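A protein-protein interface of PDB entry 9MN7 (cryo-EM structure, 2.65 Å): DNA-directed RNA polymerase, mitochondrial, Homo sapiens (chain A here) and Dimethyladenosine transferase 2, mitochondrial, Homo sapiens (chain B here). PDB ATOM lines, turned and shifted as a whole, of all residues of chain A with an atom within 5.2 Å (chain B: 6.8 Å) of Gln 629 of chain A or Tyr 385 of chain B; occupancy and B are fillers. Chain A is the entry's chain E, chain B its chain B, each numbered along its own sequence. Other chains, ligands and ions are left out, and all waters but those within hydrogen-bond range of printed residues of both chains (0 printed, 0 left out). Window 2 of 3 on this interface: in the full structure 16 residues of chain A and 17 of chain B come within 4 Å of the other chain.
ND1 of His 624 of chain A lies within hydrogen-bond range of N of Ala 626 of chain A (2.9 Å).
Of the printed residues of chain B, His 624 of chain A touches Pro 344. Of the printed residues of chain B, Pro 625 of chain A touches Tyr 385. Of the printed residues of chain B, Ala 626 of chain A touches Tyr 385. Gln 629 of chain A touches one residue of chain B. Tyr 385 of chain B touches just these residues of chain A: Pro 625, Ala 626 and Gln 629. Leu 388 of chain B touches none of the printed residues of chain A. The nearest printed residue of chain B that does not touch Gln 629 of chain A is Ala 384 of chain B (9.4 Å).
Hydrophobic or aromatic side chains of chain B that line the printed part of chain A: Pro 344 and Tyr 385. Hydrophobic or aromatic side chains of chain A within 4 Å of the printed part of chain B: His 624, Pro 625 and Ala 626. Among the printed residues, no Asp or Glu carboxylate lies within 4 Å of a Lys or Arg side-chain nitrogen of the other chain.
Among the printed residues, pairs that only touch across the chains: Pro 625 of chain A with Tyr 385 of chain B (3.6 Å), Ala 626 of chain A with Tyr 385 of chain B (3.7 Å), Gln 629 of chain A with Tyr 385 of chain B (3.8 Å) and His 624 of chain A with Pro 344 of chain B (3.96 Å).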
ATOM      1  N   HIS A 624     -20.952   5.593  -5.212  1.00  0.00           N
ATOM      2  CA  HIS A 624     -19.574   5.421  -4.785  1.00  0.00           C
ATOM      3  C   HIS A 624     -18.791   6.683  -5.146  1.00  0.00           C
ATOM      4  O   HIS A 624     -18.978   7.232  -6.239  1.00  0.00           O
ATOM      5  CB  HIS A 624     -18.976   4.192  -5.478  1.00  0.00           C
ATOM      6  CG  HIS A 624     -17.687   3.699  -4.888  1.00  0.00           C
ATOM      7  ND1 HIS A 624     -16.603   4.511  -4.643  1.00  0.00           N
ATOM      8  CD2 HIS A 624     -17.301   2.450  -4.533  1.00  0.00           C
ATOM      9  CE1 HIS A 624     -15.616   3.794  -4.139  1.00  0.00           C
ATOM     10  NE2 HIS A 624     -16.013   2.538  -4.065  1.00  0.00           N
ATOM     11  N   PRO A 625     -17.949   7.196  -4.243  1.00  0.00           N
ATOM     12  CA  PRO A 625     -17.136   8.377  -4.581  1.00  0.00           C
ATOM     13  C   PRO A 625     -16.185   8.174  -5.750  1.00  0.00           C
ATOM     14  O   PRO A 625     -15.892   9.137  -6.467  1.00  0.00           O
ATOM     15  CB  PRO A 625     -16.379   8.649  -3.276  1.00  0.00           C
ATOM     16  CG  PRO A 625     -17.324   8.187  -2.224  1.00  0.00           C
ATOM     17  CD  PRO A 625     -17.947   6.935  -2.792  1.00  0.00           C
ATOM     18  N   ALA A 626     -15.684   6.955  -5.956  1.00  0.00           N
ATOM     19  CA  ALA A 626     -14.872   6.671  -7.135  1.00  0.00           C
ATOM     20  C   ALA A 626     -15.696   6.773  -8.411  1.00  0.00           C
ATOM     21  O   ALA A 626     -15.212   7.279  -9.427  1.00  0.00           O
ATOM     22  CB  ALA A 626     -14.233   5.288  -7.021  1.00  0.00           C
ATOM     23  N   TYR A 627     -16.947   6.304  -8.373  1.00  0.00           N
ATOM     24  CA  TYR A 627     -17.847   6.470  -9.512  1.00  0.00           C
ATOM     25  C   TYR A 627     -18.137   7.941  -9.788  1.00  0.00           C
ATOM     26  O   TYR A 627     -18.173   8.363 -10.950  1.00  0.00           O
ATOM     27  CB  TYR A 627     -19.149   5.708  -9.276  1.00  0.00           C
ATOM     28  CG  TYR A 627     -20.137   5.834 -10.412  1.00  0.00           C
ATOM     29  CD1 TYR A 627     -19.814   5.413 -11.693  1.00  0.00           C
ATOM     30  CD2 TYR A 627     -21.395   6.384 -10.202  1.00  0.00           C
ATOM     31  CE1 TYR A 627     -20.714   5.537 -12.732  1.00  0.00           C
ATOM     32  CE2 TYR A 627     -22.301   6.506 -11.234  1.00  0.00           C
ATOM     33  CZ  TYR A 627     -21.954   6.080 -12.495  1.00  0.00           C
ATOM     34  OH  TYR A 627     -22.855   6.201 -13.524  1.00  0.00           O
ATOM     35  N   VAL A 628     -18.335   8.734  -8.731  1.00  0.00           N
ATOM     36  CA  VAL A 628     -18.548  10.168  -8.897  1.00  0.00           C
ATOM     37  C   VAL A 628     -17.326  10.824  -9.530  1.00  0.00           C
ATOM     38  O   VAL A 628     -17.440  11.497 -10.560  1.00  0.00           O
ATOM     39  CB  VAL A 628     -18.903  10.811  -7.546  1.00  0.00           C
ATOM     40  CG1 VAL A 628     -18.964  12.315  -7.673  1.00  0.00           C
ATOM     41  CG2 VAL A 628     -20.225  10.274  -7.042  1.00  0.00           C
ATOM     42  N   GLN A 629     -16.137  10.566  -8.971  1.00  0.00           N
ATOM     43  CA  GLN A 629     -14.892  11.113  -9.505  1.00  0.00           C
ATOM     44  C   GLN A 629     -14.647  10.657 -10.942  1.00  0.00           C
ATOM     45  O   GLN A 629     -14.069  11.397 -11.746  1.00  0.00           O
ATOM     46  CB  GLN A 629     -13.736  10.709  -8.587  1.00  0.00           C
ATOM     47  CG  GLN A 629     -12.384  11.334  -8.887  1.00  0.00           C
ATOM     48  CD  GLN A 629     -11.557  10.511  -9.853  1.00  0.00           C
ATOM     49  OE1 GLN A 629     -11.687   9.288  -9.916  1.00  0.00           O
ATOM     50  NE2 GLN A 629     -10.692  11.177 -10.604  1.00  0.00           N
ATOM     51  N   LEU A 630     -15.112   9.455 -11.289  1.00  0.00           N
ATOM     52  CA  LEU A 630     -15.101   9.014 -12.677  1.00  0.00           C
ATOM     53  C   LEU A 630     -16.048   9.849 -13.530  1.00  0.00           C
ATOM     54  O   LEU A 630     -15.764  10.112 -14.704  1.00  0.00           O
ATOM     55  CB  LEU A 630     -15.470   7.533 -12.747  1.00  0.00           C
ATOM     56  CG  LEU A 630     -15.462   6.829 -14.102  1.00  0.00           C
ATOM     57  CD1 LEU A 630     -14.072   6.831 -14.691  1.00  0.00           C
ATOM     58  CD2 LEU A 630     -15.981   5.406 -13.960  1.00  0.00           C
ATOM     59  N   LEU A 631     -17.188  10.263 -12.964  1.00  0.00           N
ATOM     60  CA  LEU A 631     -18.126  11.082 -13.732  1.00  0.00           C
ATOM     61  C   LEU A 631     -17.588  12.487 -13.998  1.00  0.00           C
ATOM     62  O   LEU A 631     -17.655  12.963 -15.136  1.00  0.00           O
ATOM     63  CB  LEU A 631     -19.489  11.151 -13.043  1.00  0.00           C
ATOM     64  CG  LEU A 631     -20.285   9.851 -12.951  1.00  0.00           C
ATOM     65  CD1 LEU A 631     -21.544  10.049 -12.125  1.00  0.00           C
ATOM     66  CD2 LEU A 631     -20.625   9.338 -14.339  1.00  0.00           C
ATOM     67  N   GLU A 632     -17.070  13.184 -12.977  1.00  0.00           N
ATOM     68  CA  GLU A 632     -16.531  14.518 -13.283  1.00  0.00           C
ATOM     69  C   GLU A 632     -15.179  14.461 -13.988  1.00  0.00           C
ATOM     70  O   GLU A 632     -14.808  15.423 -14.670  1.00  0.00           O
ATOM     71  CB  GLU A 632     -16.430  15.487 -12.088  1.00  0.00           C
ATOM     72  CG  GLU A 632     -17.727  16.016 -11.443  1.00  0.00           C
ATOM     73  CD  GLU A 632     -18.352  15.125 -10.422  1.00  0.00           C
ATOM     74  OE1 GLU A 632     -17.754  14.096 -10.127  1.00  0.00           O
ATOM     75  OE2 GLU A 632     -19.442  15.458  -9.910  1.00  0.00           O
ATOM     76  N   LYS A 633     -14.416  13.376 -13.842  1.00  0.00           N
ATOM     77  CA  LYS A 633     -13.152  13.326 -14.573  1.00  0.00           C
ATOM     78  C   LYS A 633     -13.389  13.109 -16.064  1.00  0.00           C
ATOM     79  O   LYS A 633     -12.785  13.792 -16.900  1.00  0.00           O
ATOM     80  CB  LYS A 633     -12.230  12.251 -13.996  1.00  0.00           C
ATOM     81  CG  LYS A 633     -11.159  11.778 -14.971  1.00  0.00           C
ATOM     82  CD  LYS A 633     -10.007  11.088 -14.273  1.00  0.00           C
ATOM     83  CE  LYS A 633      -9.201  12.082 -13.452  1.00  0.00           C
ATOM     84  NZ  LYS A 633      -7.986  11.463 -12.853  1.00  0.00           N
ATOM     85  N   ALA A 634     -14.286  12.195 -16.417  1.00  0.00           N
ATOM     86  CA  ALA A 634     -14.710  12.011 -17.802  1.00  0.00           C
ATOM     87  C   ALA A 634     -15.965  12.851 -17.996  1.00  0.00           C
ATOM     88  O   ALA A 634     -17.087  12.359 -17.869  1.00  0.00           O
ATOM     89  CB  ALA A 634     -14.961  10.541 -18.114  1.00  0.00           C
ATOM     90  N   THR B 343     -19.289   2.483   4.630  1.00  0.00           N
ATOM     91  CA  THR B 343     -17.878   2.531   4.278  1.00  0.00           C
ATOM     92  C   THR B 343     -17.668   1.604   3.090  1.00  0.00           C
ATOM     93  O   THR B 343     -18.229   0.499   3.074  1.00  0.00           O
ATOM     94  CB  THR B 343     -17.005   2.088   5.466  1.00  0.00           C
ATOM     95  OG1 THR B 343     -17.226   2.957   6.585  1.00  0.00           O
ATOM     96  CG2 THR B 343     -15.530   2.102   5.136  1.00  0.00           C
ATOM     97  N   PRO B 344     -16.880   2.012   2.093  1.00  0.00           N
ATOM     98  CA  PRO B 344     -16.558   1.115   0.978  1.00  0.00           C
ATOM     99  C   PRO B 344     -15.421   0.146   1.259  1.00  0.00           C
ATOM    100  O   PRO B 344     -15.074  -0.644   0.372  1.00  0.00           O
ATOM    101  CB  PRO B 344     -16.171   2.093  -0.135  1.00  0.00           C
ATOM    102  CG  PRO B 344     -15.584   3.240   0.587  1.00  0.00           C
ATOM    103  CD  PRO B 344     -16.348   3.369   1.877  1.00  0.00           C
ATOM    104  N   LEU B 345     -14.827   0.188   2.448  1.00  0.00           N
ATOM    105  CA  LEU B 345     -13.761  -0.739   2.785  1.00  0.00           C
ATOM    106  C   LEU B 345     -14.322  -2.118   3.109  1.00  0.00           C
ATOM    107  O   LEU B 345     -15.511  -2.289   3.392  1.00  0.00           O
ATOM    108  CB  LEU B 345     -12.944  -0.228   3.969  1.00  0.00           C
ATOM    109  CG  LEU B 345     -12.141   1.028   3.656  1.00  0.00           C
ATOM    110  CD1 LEU B 345     -11.411   1.534   4.881  1.00  0.00           C
ATOM    111  CD2 LEU B 345     -11.169   0.728   2.540  1.00  0.00           C
ATOM    112  N   ILE B 377     -10.133   2.680  10.634  1.00  0.00           N
ATOM    113  CA  ILE B 377     -10.309   3.024   9.228  1.00  0.00           C
ATOM    114  C   ILE B 377      -9.250   4.028   8.782  1.00  0.00           C
ATOM    115  O   ILE B 377      -8.762   3.974   7.645  1.00  0.00           O
ATOM    116  CB  ILE B 377     -11.742   3.550   9.013  1.00  0.00           C
ATOM    117  CG1 ILE B 377     -12.752   2.460   9.368  1.00  0.00           C
ATOM    118  CG2 ILE B 377     -11.968   4.020   7.584  1.00  0.00           C
ATOM    119  CD1 ILE B 377     -14.181   2.936   9.397  1.00  0.00           C
ATOM    120  N   ASP B 382      -3.720   4.463   1.944  1.00  0.00           N
ATOM    121  CA  ASP B 382      -3.821   4.175   0.516  1.00  0.00           C
ATOM    122  C   ASP B 382      -5.264   4.258   0.028  1.00  0.00           C
ATOM    123  O   ASP B 382      -5.525   4.719  -1.089  1.00  0.00           O
ATOM    124  CB  ASP B 382      -3.222   2.800   0.214  1.00  0.00           C
ATOM    125  CG  ASP B 382      -3.744   1.715   1.140  1.00  0.00           C
ATOM    126  OD1 ASP B 382      -4.543   2.029   2.048  1.00  0.00           O
ATOM    127  OD2 ASP B 382      -3.351   0.543   0.960  1.00  0.00           O
ATOM    128  N   CYS B 383      -6.211   3.813   0.850  1.00  0.00           N
ATOM    129  CA  CYS B 383      -7.632   3.875   0.514  1.00  0.00           C
ATOM    130  C   CYS B 383      -8.157   5.252   0.900  1.00  0.00           C
ATOM    131  O   CYS B 383      -8.526   5.504   2.048  1.00  0.00           O
ATOM    132  CB  CYS B 383      -8.397   2.764   1.218  1.00  0.00           C
ATOM    133  SG  CYS B 383      -7.940   1.099   0.681  1.00  0.00           S
ATOM    134  N   ALA B 384      -8.184   6.159  -0.081  1.00  0.00           N
ATOM    135  CA  ALA B 384      -8.610   7.532   0.181  1.00  0.00           C
ATOM    136  C   ALA B 384     -10.109   7.618   0.449  1.00  0.00           C
ATOM    137  O   ALA B 384     -10.550   8.423   1.276  1.00  0.00           O
ATOM    138  CB  ALA B 384      -8.222   8.431  -0.993  1.00  0.00           C
ATOM    139  N   TYR B 385     -10.906   6.806  -0.241  1.00  0.00           N
ATOM    140  CA  TYR B 385     -12.358   6.831  -0.084  1.00  0.00           C
ATOM    141  C   TYR B 385     -12.701   6.053   1.176  1.00  0.00           C
ATOM    142  O   TYR B 385     -12.710   4.819   1.179  1.00  0.00           O
ATOM    143  CB  TYR B 385     -13.038   6.245  -1.315  1.00  0.00           C
ATOM    144  CG  TYR B 385     -12.650   6.943  -2.601  1.00  0.00           C
ATOM    145  CD1 TYR B 385     -12.811   8.317  -2.746  1.00  0.00           C
ATOM    146  CD2 TYR B 385     -12.104   6.230  -3.660  1.00  0.00           C
ATOM    147  CE1 TYR B 385     -12.452   8.958  -3.920  1.00  0.00           C
ATOM    148  CE2 TYR B 385     -11.741   6.863  -4.835  1.00  0.00           C
ATOM    149  CZ  TYR B 385     -11.917   8.225  -4.957  1.00  0.00           C
ATOM    150  OH  TYR B 385     -11.558   8.858  -6.124  1.00  0.00           O
ATOM    151  N   LYS B 386     -12.986   6.776   2.256  1.00  0.00           N
ATOM    152  CA  LYS B 386     -13.106   6.191   3.586  1.00  0.00           C
ATOM    153  C   LYS B 386     -14.532   6.176   4.119  1.00  0.00           C
ATOM    154  O   LYS B 386     -14.897   5.261   4.859  1.00  0.00           O
ATOM    155  CB  LYS B 386     -12.201   6.946   4.566  1.00  0.00           C
ATOM    156  CG  LYS B 386     -10.721   6.816   4.250  1.00  0.00           C
ATOM    157  CD  LYS B 386      -9.848   7.133   5.456  1.00  0.00           C
ATOM    158  CE  LYS B 386     -10.125   8.530   5.997  1.00  0.00           C
ATOM    159  NZ  LYS B 386      -9.216   8.879   7.127  1.00  0.00           N
ATOM    160  N   TRP B 387     -15.351   7.161   3.760  1.00  0.00           N
ATOM    161  CA  TRP B 387     -16.657   7.325   4.379  1.00  0.00           C
ATOM    162  C   TRP B 387     -17.689   7.705   3.329  1.00  0.00           C
ATOM    163  O   TRP B 387     -17.357   8.023   2.184  1.00  0.00           O
ATOM    164  CB  TRP B 387     -16.623   8.400   5.469  1.00  0.00           C
ATOM    165  CG  TRP B 387     -15.790   8.027   6.644  1.00  0.00           C
ATOM    166  CD1 TRP B 387     -14.491   8.376   6.869  1.00  0.00           C
ATOM    167  CD2 TRP B 387     -16.193   7.232   7.762  1.00  0.00           C
ATOM    168  NE1 TRP B 387     -14.059   7.844   8.058  1.00  0.00           N
ATOM    169  CE2 TRP B 387     -15.085   7.137   8.626  1.00  0.00           C
ATOM    170  CE3 TRP B 387     -17.384   6.590   8.116  1.00  0.00           C
ATOM    171  CZ2 TRP B 387     -15.134   6.428   9.821  1.00  0.00           C
ATOM    172  CZ3 TRP B 387     -17.428   5.887   9.305  1.00  0.00           C
ATOM    173  CH2 TRP B 387     -16.311   5.812  10.142  1.00  0.00           C
ATOM    174  N   LEU B 388     -18.954   7.662   3.738  1.00  0.00           N
ATOM    175  CA  LEU B 388     -20.070   8.179   2.958  1.00  0.00           C
ATOM    176  C   LEU B 388     -20.912   9.146   3.780  1.00  0.00           C
ATOM    177  O   LEU B 388     -22.141   9.058   3.808  1.00  0.00           O
ATOM    178  CB  LEU B 388     -20.949   7.057   2.405  1.00  0.00           C
ATOM    179  CG  LEU B 388     -20.524   6.382   1.098  1.00  0.00           C
ATOM    180  CD1 LEU B 388     -19.399   5.384   1.292  1.00  0.00           C
ATOM    181  CD2 LEU B 388     -21.717   5.734   0.419  1.00  0.00           C
